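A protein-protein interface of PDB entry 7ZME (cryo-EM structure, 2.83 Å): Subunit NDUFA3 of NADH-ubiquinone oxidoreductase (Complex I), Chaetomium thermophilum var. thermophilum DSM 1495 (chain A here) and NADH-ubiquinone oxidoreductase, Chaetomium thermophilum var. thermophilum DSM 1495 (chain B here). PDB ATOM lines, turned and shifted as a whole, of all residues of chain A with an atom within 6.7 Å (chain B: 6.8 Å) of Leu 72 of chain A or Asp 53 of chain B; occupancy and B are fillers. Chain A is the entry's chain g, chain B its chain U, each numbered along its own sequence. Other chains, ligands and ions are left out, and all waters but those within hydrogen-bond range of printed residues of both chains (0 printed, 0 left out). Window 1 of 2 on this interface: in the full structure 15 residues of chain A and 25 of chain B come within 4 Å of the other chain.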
ATOM      1  N   TYR A  62     -18.461  27.781  15.766  1.00  0.00           N
ATOM      2  CA  TYR A  62     -17.567  27.175  16.779  1.00  0.00           C
ATOM      3  C   TYR A  62     -18.349  27.002  18.077  1.00  0.00           C
ATOM      4  O   TYR A  62     -18.957  27.964  18.564  1.00  0.00           O
ATOM      5  CB  TYR A  62     -16.321  28.032  17.011  1.00  0.00           C
ATOM      6  CG  TYR A  62     -15.239  27.353  17.810  1.00  0.00           C
ATOM      7  CD1 TYR A  62     -15.279  27.321  19.195  1.00  0.00           C
ATOM      8  CD2 TYR A  62     -14.176  26.733  17.180  1.00  0.00           C
ATOM      9  CE1 TYR A  62     -14.297  26.683  19.932  1.00  0.00           C
ATOM     10  CE2 TYR A  62     -13.181  26.099  17.902  1.00  0.00           C
ATOM     11  CZ  TYR A  62     -13.241  26.074  19.282  1.00  0.00           C
ATOM     12  OH  TYR A  62     -12.259  25.453  19.994  1.00  0.00           O
ATOM     13  N   PRO A  65     -17.473  26.776  24.720  1.00  0.00           N
ATOM     14  CA  PRO A  65     -17.913  26.121  25.946  1.00  0.00           C
ATOM     15  C   PRO A  65     -18.385  27.143  26.963  1.00  0.00           C
ATOM     16  O   PRO A  65     -17.934  28.300  26.957  1.00  0.00           O
ATOM     17  CB  PRO A  65     -16.646  25.391  26.431  1.00  0.00           C
ATOM     18  CG  PRO A  65     -15.686  25.450  25.285  1.00  0.00           C
ATOM     19  CD  PRO A  65     -16.018  26.689  24.544  1.00  0.00           C
ATOM     20  N   ARG A  69     -12.911  30.176  32.448  1.00  0.00           N
ATOM     21  CA  ARG A  69     -11.758  29.630  31.751  1.00  0.00           C
ATOM     22  C   ARG A  69     -10.995  28.663  32.655  1.00  0.00           C
ATOM     23  O   ARG A  69     -11.078  28.721  33.885  1.00  0.00           O
ATOM     24  CB  ARG A  69     -10.845  30.757  31.268  1.00  0.00           C
ATOM     25  CG  ARG A  69     -11.466  31.596  30.158  1.00  0.00           C
ATOM     26  CD  ARG A  69     -10.670  32.856  29.888  1.00  0.00           C
ATOM     27  NE  ARG A  69      -9.360  32.562  29.327  1.00  0.00           N
ATOM     28  CZ  ARG A  69      -8.476  33.484  28.966  1.00  0.00           C
ATOM     29  NH1 ARG A  69      -7.308  33.118  28.461  1.00  0.00           N
ATOM     30  NH2 ARG A  69      -8.760  34.769  29.111  1.00  0.00           N
ATOM     31  N   LYS A  70     -10.246  27.760  32.026  1.00  0.00           N
ATOM     32  CA  LYS A  70      -9.713  26.589  32.711  1.00  0.00           C
ATOM     33  C   LYS A  70      -8.318  26.789  33.290  1.00  0.00           C
ATOM     34  O   LYS A  70      -7.784  25.851  33.890  1.00  0.00           O
ATOM     35  CB  LYS A  70      -9.709  25.387  31.762  1.00  0.00           C
ATOM     36  CG  LYS A  70     -10.992  24.578  31.802  1.00  0.00           C
ATOM     37  CD  LYS A  70     -11.120  23.674  30.589  1.00  0.00           C
ATOM     38  CE  LYS A  70     -10.383  22.367  30.798  1.00  0.00           C
ATOM     39  NZ  LYS A  70     -11.140  21.443  31.686  1.00  0.00           N
ATOM     40  N   GLN A  71      -7.718  27.971  33.134  1.00  0.00           N
ATOM     41  CA  GLN A  71      -6.460  28.324  33.801  1.00  0.00           C
ATOM     42  C   GLN A  71      -5.370  27.288  33.496  1.00  0.00           C
ATOM     43  O   GLN A  71      -4.895  26.555  34.363  1.00  0.00           O
ATOM     44  CB  GLN A  71      -6.678  28.479  35.312  1.00  0.00           C
ATOM     45  CG  GLN A  71      -5.520  29.126  36.055  1.00  0.00           C
ATOM     46  CD  GLN A  71      -5.271  30.555  35.612  1.00  0.00           C
ATOM     47  OE1 GLN A  71      -4.361  30.825  34.830  1.00  0.00           O
ATOM     48  NE2 GLN A  71      -6.081  31.480  36.115  1.00  0.00           N
ATOM     49  N   LEU A  72      -5.002  27.242  32.222  1.00  0.00           N
ATOM     50  CA  LEU A  72      -4.107  26.218  31.708  1.00  0.00           C
ATOM     51  C   LEU A  72      -2.645  26.612  31.869  1.00  0.00           C
ATOM     52  O   LEU A  72      -2.297  27.795  31.915  1.00  0.00           O
ATOM     53  CB  LEU A  72      -4.404  25.948  30.235  1.00  0.00           C
ATOM     54  CG  LEU A  72      -5.736  25.262  29.966  1.00  0.00           C
ATOM     55  CD1 LEU A  72      -6.313  25.749  28.669  1.00  0.00           C
ATOM     56  CD2 LEU A  72      -5.526  23.767  29.928  1.00  0.00           C
ATOM     57  N   LYS A  73      -1.787  25.597  31.956  1.00  0.00           N
ATOM     58  CA  LYS A  73      -0.342  25.778  32.050  1.00  0.00           C
ATOM     59  C   LYS A  73       0.329  24.789  31.109  1.00  0.00           C
ATOM     60  O   LYS A  73       0.299  23.579  31.356  1.00  0.00           O
ATOM     61  CB  LYS A  73       0.153  25.571  33.485  1.00  0.00           C
ATOM     62  CG  LYS A  73      -0.488  26.487  34.514  1.00  0.00           C
ATOM     63  CD  LYS A  73       0.275  26.460  35.830  1.00  0.00           C
ATOM     64  CE  LYS A  73       0.440  25.039  36.345  1.00  0.00           C
ATOM     65  NZ  LYS A  73      -0.872  24.377  36.585  1.00  0.00           N
ATOM     66  N   GLY A  74       0.847  25.309  29.995  1.00  0.00           N
ATOM     67  CA  GLY A  74       1.511  24.485  28.967  1.00  0.00           C
ATOM     68  C   GLY A  74       1.818  25.291  27.738  1.00  0.00           C
ATOM     69  O   GLY A  74       1.216  26.352  27.606  1.00  0.00           O
ATOM     70  N   ASP A  76       3.891  27.397  26.825  1.00  0.00           N
ATOM     71  CA  ASP A  76       4.146  28.833  27.091  1.00  0.00           C
ATOM     72  C   ASP A  76       5.321  29.297  26.230  1.00  0.00           C
ATOM     73  O   ASP A  76       5.872  28.473  25.495  1.00  0.00           O
ATOM     74  CB  ASP A  76       4.339  29.086  28.585  1.00  0.00           C
ATOM     75  CG  ASP A  76       3.037  29.028  29.364  1.00  0.00           C
ATOM     76  OD1 ASP A  76       1.973  29.203  28.736  1.00  0.00           O
ATOM     77  OD2 ASP A  76       3.096  28.807  30.589  1.00  0.00           O
ATOM     78  N   CYS B  47      -5.221  19.200  22.039  1.00  0.00           N
ATOM     79  CA  CYS B  47      -5.170  20.652  22.142  1.00  0.00           C
ATOM     80  C   CYS B  47      -6.535  21.280  22.399  1.00  0.00           C
ATOM     81  O   CYS B  47      -6.678  22.497  22.253  1.00  0.00           O
ATOM     82  CB  CYS B  47      -4.554  21.235  20.872  1.00  0.00           C
ATOM     83  SG  CYS B  47      -2.855  20.719  20.596  1.00  0.00           S
ATOM     84  N   LYS B  48      -7.533  20.482  22.785  1.00  0.00           N
ATOM     85  CA  LYS B  48      -8.888  21.005  22.930  1.00  0.00           C
ATOM     86  C   LYS B  48      -8.961  22.110  23.975  1.00  0.00           C
ATOM     87  O   LYS B  48      -9.598  23.143  23.749  1.00  0.00           O
ATOM     88  CB  LYS B  48      -9.852  19.877  23.291  1.00  0.00           C
ATOM     89  CG  LYS B  48     -11.307  20.305  23.358  1.00  0.00           C
ATOM     90  CD  LYS B  48     -12.218  19.123  23.640  1.00  0.00           C
ATOM     91  CE  LYS B  48     -13.674  19.550  23.715  1.00  0.00           C
ATOM     92  NZ  LYS B  48     -14.572  18.396  23.994  1.00  0.00           N
ATOM     93  N   ASP B  49      -8.315  21.910  25.125  1.00  0.00           N
ATOM     94  CA  ASP B  49      -8.415  22.883  26.209  1.00  0.00           C
ATOM     95  C   ASP B  49      -7.841  24.231  25.798  1.00  0.00           C
ATOM     96  O   ASP B  49      -8.401  25.280  26.133  1.00  0.00           O
ATOM     97  CB  ASP B  49      -7.703  22.353  27.451  1.00  0.00           C
ATOM     98  CG  ASP B  49      -8.383  21.136  28.032  1.00  0.00           C
ATOM     99  OD1 ASP B  49      -9.626  21.059  27.957  1.00  0.00           O
ATOM    100  OD2 ASP B  49      -7.676  20.255  28.564  1.00  0.00           O
ATOM    101  N   TYR B  50      -6.733  24.208  25.059  1.00  0.00           N
ATOM    102  CA  TYR B  50      -6.072  25.449  24.591  1.00  0.00           C
ATOM    103  C   TYR B  50      -6.863  26.021  23.416  1.00  0.00           C
ATOM    104  O   TYR B  50      -7.027  27.242  23.342  1.00  0.00           O
ATOM    105  CB  TYR B  50      -4.624  25.117  24.226  1.00  0.00           C
ATOM    106  CG  TYR B  50      -3.834  24.508  25.355  1.00  0.00           C
ATOM    107  CD1 TYR B  50      -3.168  25.306  26.267  1.00  0.00           C
ATOM    108  CD2 TYR B  50      -3.762  23.135  25.523  1.00  0.00           C
ATOM    109  CE1 TYR B  50      -2.439  24.761  27.309  1.00  0.00           C
ATOM    110  CE2 TYR B  50      -3.043  22.573  26.563  1.00  0.00           C
ATOM    111  CZ  TYR B  50      -2.377  23.389  27.458  1.00  0.00           C
ATOM    112  OH  TYR B  50      -1.662  22.843  28.483  1.00  0.00           O
ATOM    113  N   ASN B  51      -7.361  25.152  22.539  1.00  0.00           N
ATOM    114  CA  ASN B  51      -8.203  25.600  21.403  1.00  0.00           C
ATOM    115  C   ASN B  51      -9.449  26.272  21.972  1.00  0.00           C
ATOM    116  O   ASN B  51      -9.877  27.284  21.407  1.00  0.00           O
ATOM    117  CB  ASN B  51      -8.613  24.436  20.502  1.00  0.00           C
ATOM    118  CG  ASN B  51      -7.548  24.028  19.511  1.00  0.00           C
ATOM    119  OD1 ASN B  51      -6.556  24.731  19.331  1.00  0.00           O
ATOM    120  ND2 ASN B  51      -7.750  22.896  18.859  1.00  0.00           N
ATOM    121  N   ASP B  52      -9.980  25.746  23.071  1.00  0.00           N
ATOM    122  CA  ASP B  52     -11.222  26.294  23.671  1.00  0.00           C
ATOM    123  C   ASP B  52     -10.878  27.513  24.519  1.00  0.00           C
ATOM    124  O   ASP B  52     -11.733  28.392  24.632  1.00  0.00           O
ATOM    125  CB  ASP B  52     -11.947  25.233  24.495  1.00  0.00           C
ATOM    126  CG  ASP B  52     -12.680  24.195  23.665  1.00  0.00           C
ATOM    127  OD1 ASP B  52     -12.871  24.436  22.464  1.00  0.00           O
ATOM    128  OD2 ASP B  52     -13.056  23.156  24.234  1.00  0.00           O
ATOM    129  N   ASP B  53      -9.663  27.575  25.059  1.00  0.00           N
ATOM    130  CA  ASP B  53      -9.260  28.703  25.937  1.00  0.00           C
ATOM    131  C   ASP B  53      -9.037  29.922  25.059  1.00  0.00           C
ATOM    132  O   ASP B  53      -9.493  31.008  25.443  1.00  0.00           O
ATOM    133  CB  ASP B  53      -7.959  28.413  26.675  1.00  0.00           C
ATOM    134  CG  ASP B  53      -7.657  29.384  27.802  1.00  0.00           C
ATOM    135  OD1 ASP B  53      -8.571  29.652  28.603  1.00  0.00           O
ATOM    136  OD2 ASP B  53      -6.510  29.861  27.867  1.00  0.00           O
ATOM    137  N   TYR B  54      -8.442  29.769  23.877  1.00  0.00           N
ATOM    138  CA  TYR B  54      -8.160  30.962  23.041  1.00  0.00           C
ATOM    139  C   TYR B  54      -9.483  31.562  22.548  1.00  0.00           C
ATOM    140  O   TYR B  54      -9.564  32.796  22.443  1.00  0.00           O
ATOM    141  CB  TYR B  54      -7.269  30.543  21.871  1.00  0.00           C
ATOM    142  CG  TYR B  54      -7.096  31.545  20.760  1.00  0.00           C
ATOM    143  CD1 TYR B  54      -6.413  32.730  20.968  1.00  0.00           C
ATOM    144  CD2 TYR B  54      -7.598  31.299  19.493  1.00  0.00           C
ATOM    145  CE1 TYR B  54      -6.242  33.653  19.951  1.00  0.00           C
ATOM    146  CE2 TYR B  54      -7.437  32.210  18.465  1.00  0.00           C
ATOM    147  CZ  TYR B  54      -6.752  33.389  18.695  1.00  0.00           C
ATOM    148  OH  TYR B  54      -6.583  34.299  17.695  1.00  0.00           O
ATOM    149  N   MET B  55     -10.483  30.728  22.282  1.00  0.00           N
ATOM    150  CA  MET B  55     -11.804  31.181  21.768  1.00  0.00           C
ATOM    151  C   MET B  55     -12.609  31.888  22.857  1.00  0.00           C
ATOM    152  O   MET B  55     -13.335  32.830  22.522  1.00  0.00           O
ATOM    153  CB  MET B  55     -12.575  30.006  21.161  1.00  0.00           C
ATOM    154  CG  MET B  55     -11.873  29.376  19.978  1.00  0.00           C
ATOM    155  SD  MET B  55     -11.675  30.497  18.578  1.00  0.00           S
ATOM    156  CE  MET B  55     -13.330  30.480  17.894  1.00  0.00           C
ATOM    157  N   GLN B  56     -12.486  31.426  24.103  1.00  0.00           N
ATOM    158  CA  GLN B  56     -13.190  32.038  25.259  1.00  0.00           C
ATOM    159  C   GLN B  56     -12.445  33.316  25.638  1.00  0.00           C
ATOM    160  O   GLN B  56     -13.103  34.228  26.154  1.00  0.00           O
ATOM    161  CB  GLN B  56     -13.208  31.080  26.444  1.00  0.00           C
ATOM    162  CG  GLN B  56     -14.097  29.862  26.258  1.00  0.00           C
ATOM    163  CD  GLN B  56     -13.774  28.805  27.284  1.00  0.00           C
ATOM    164  OE1 GLN B  56     -14.523  27.854  27.482  1.00  0.00           O
ATOM    165  NE2 GLN B  56     -12.645  28.970  27.952  1.00  0.00           N
ATOM    166  N   CYS B  57     -11.137  33.395  25.370  1.00  0.00           N
ATOM    167  CA  CYS B  57     -10.447  34.660  25.589  1.00  0.00           C
ATOM    168  C   CYS B  57     -10.974  35.739  24.655  1.00  0.00           C
ATOM    169  O   CYS B  57     -11.252  36.865  25.079  1.00  0.00           O
ATOM    170  CB  CYS B  57      -8.941  34.470  25.395  1.00  0.00           C
ATOM    171  SG  CYS B  57      -7.947  35.973  25.533  1.00  0.00           S
ATOM    172  N   LYS B  58     -11.115  35.409  23.370  1.00  0.00           N
ATOM    173  CA  LYS B  58     -11.571  36.397  22.400  1.00  0.00           C
ATOM    174  C   LYS B  58     -12.995  36.840  22.692  1.00  0.00           C
ATOM    175  O   LYS B  58     -13.324  38.021  22.545  1.00  0.00           O
ATOM    176  CB  LYS B  58     -11.449  35.838  20.987  1.00  0.00           C
ATOM    177  CG  LYS B  58     -10.019  35.736  20.507  1.00  0.00           C
ATOM    178  CD  LYS B  58      -9.936  35.077  19.156  1.00  0.00           C
ATOM    179  CE  LYS B  58      -9.936  36.104  18.046  1.00  0.00           C
ATOM    180  NZ  LYS B  58      -9.572  35.479  16.748  1.00  0.00           N
ATOM    181  N   CYS B  69      -5.398  38.625  22.922  1.00  0.00           N
ATOM    182  CA  CYS B  69      -5.273  37.166  23.201  1.00  0.00           C
ATOM    183  C   CYS B  69      -4.077  36.579  22.438  1.00  0.00           C
ATOM    184  O   CYS B  69      -4.153  35.402  22.046  1.00  0.00           O
ATOM    185  CB  CYS B  69      -6.545  36.408  22.840  1.00  0.00           C
ATOM    186  SG  CYS B  69      -8.028  36.938  23.735  1.00  0.00           S
ATOM    187  N   GLU B  72      -2.460  33.276  24.222  1.00  0.00           N
ATOM    188  CA  GLU B  72      -3.290  32.059  24.076  1.00  0.00           C
ATOM    189  C   GLU B  72      -3.104  31.514  22.662  1.00  0.00           C
ATOM    190  O   GLU B  72      -3.018  30.296  22.524  1.00  0.00           O
ATOM    191  CB  GLU B  72      -4.743  32.383  24.416  1.00  0.00           C
ATOM    192  CG  GLU B  72      -4.987  32.666  25.886  1.00  0.00           C
ATOM    193  CD  GLU B  72      -4.545  34.031  26.389  1.00  0.00           C
ATOM    194  OE1 GLU B  72      -4.314  34.924  25.554  1.00  0.00           O
ATOM    195  OE2 GLU B  72      -4.430  34.191  27.619  1.00  0.00           O
ATOM    196  N   ARG B  75       0.105  29.760  22.309  1.00  0.00           N
ATOM    197  CA  ARG B  75      -0.032  28.458  23.012  1.00  0.00           C
ATOM    198  C   ARG B  75      -0.711  27.433  22.099  1.00  0.00           C
ATOM    199  O   ARG B  75      -0.289  26.273  22.114  1.00  0.00           O
ATOM    200  CB  ARG B  75      -0.840  28.687  24.289  1.00  0.00           C
ATOM    201  CG  ARG B  75      -0.501  27.782  25.459  1.00  0.00           C
ATOM    202  CD  ARG B  75      -1.308  28.274  26.641  1.00  0.00           C
ATOM    203  NE  ARG B  75      -1.198  29.713  26.819  1.00  0.00           N
ATOM    204  CZ  ARG B  75      -2.142  30.468  27.366  1.00  0.00           C
ATOM    205  NH1 ARG B  75      -1.959  31.771  27.496  1.00  0.00           N
ATOM    206  NH2 ARG B  75      -3.273  29.919  27.769  1.00  0.00           N
ATOM    207  N   VAL B  76      -1.734  27.839  21.351  1.00  0.00           N
ATOM    208  CA  VAL B  76      -2.459  26.864  20.480  1.00  0.00           C
ATOM    209  C   VAL B  76      -1.506  26.417  19.369  1.00  0.00           C
ATOM    210  O   VAL B  76      -1.527  25.230  19.022  1.00  0.00           O
ATOM    211  CB  VAL B  76      -3.819  27.366  19.941  1.00  0.00           C
ATOM    212  CG1 VAL B  76      -4.675  27.999  21.016  1.00  0.00           C
ATOM    213  CG2 VAL B  76      -3.696  28.281  18.737  1.00  0.00           C
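Among the printed residues, pairs that only touch across the chains: Tyr 62 of chain A with Met 55 of chain B (3.6 Å), Pro 65 of chain A with Asp 52 of chain B (3.6 Å), Arg 69 of chain A with Gln 56 of chain B (3.6 Å), Arg 69 of chain A with Cys 57 of chain B (3.7 Å), Lys 70 of chain A with Asp 49 of chain B (3.2 Å), Leu 72 of chain A with Asp 49 of chain B (3.3 Å), Leu 72 of chain A with Tyr 50 of chain B (3.7 Å), Leu 72 of chain A with Asp 53 of chain B (3.7 Å), Lys 73 of chain A with Tyr 50 of chain B (3.6 Å), Gly 74 of chain A with Tyr 50 of chain B (3.6 Å) and Gly 74 of chain A with Arg 75 of chain B (3.1 Å).
The guanidinium group of Arg 69 of chain A lies within salt-bridge range of the side-chain carboxylate of Glu 72 of chain B, 3.2 Å away. The side-chain carboxylate of Asp 52 of chain B sits at hydrogen-bond distance from the side-chain hydroxyl of Tyr 62 of chain A, at 2.7 Å. The guanidinium group (NE) of Arg 69 of chain A is in salt-bridge range of the side-chain carboxylate (OD1) of Asp 53 of chain B (3.1 Å). OE1 of Gln 56 of chain B sits close to O of Pro 65 of chain A (3.5 Å). O of Asn 51 of chain B lies within hydrogen-bond range of OH of Tyr 62 of chain A (3.3 Å). The guanidinium group (NE) of Arg 75 of chain B is in salt-bridge range of the side-chain carboxylate (OD1) of Asp 76 of chain A (3.7 Å).
Of the 16 printed residues of chain B, 10 touch a printed residue of chain A. Hydrophobic or aromatic side chains of chain B within 4 Å of the printed part of chain A: Tyr 50 and Met 55. Of the 9 printed residues of chain A, 8 touch a printed residue of chain B. Hydrophobic or aromatic side chains of chain A within 4 Å of the printed part of chain B: Tyr 62, Pro 65 and Leu 72. Among the printed residues, Asp or Glu carboxylates within 4 Å of a Lys or Arg side-chain nitrogen of the other chain: Arg 69 of chain A with Asp 53 of chain B, Arg 69 of chain A with Glu 72 of chain B and Asp 76 of chain A with Arg 75 of chain B.
Leu 72 of chain A touches just these residues of chain B: Asp 49 (3.3 Å), Tyr 50 (3.7 Å) and Asp 53 (3.7 Å). Of the printed residues of chain A, Asp 53 of chain B touches Arg 69 and Leu 72. Of the printed residues of chain B, Asp 76 of chain A touches Arg 75. Printed residues of chain B within 4 Å of Lys 70 of chain A: Asp 49 (3.2 Å). Printed residues of chain A within 4 Å of Cys 57 of chain B: Arg 69 (3.7 Å). Cys 47 of chain B touches none of the printed residues of chain A. The nearest printed residue of chain A that does not touch Asp 49 of chain B is Tyr 62 of chain A (7.3 Å).
NH2 of Arg 75 of chain B lies within salt-bridge range of OD2 of Asp 53 of chain B (3.2 Å). NE2 of Gln 56 of chain B lies close to O of Asp 52 of chain B (3.5 Å). The side-chain carboxylate of Glu 72 of chain B is in salt-bridge range of the guanidinium group of Arg 75 of chain B (3.5 Å). The side-chain sulfur (SG) of Cys 69 of chain B forms a disulfide with the side-chain sulfur (SG) of Cys 57 of chain B (2.0 Å).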
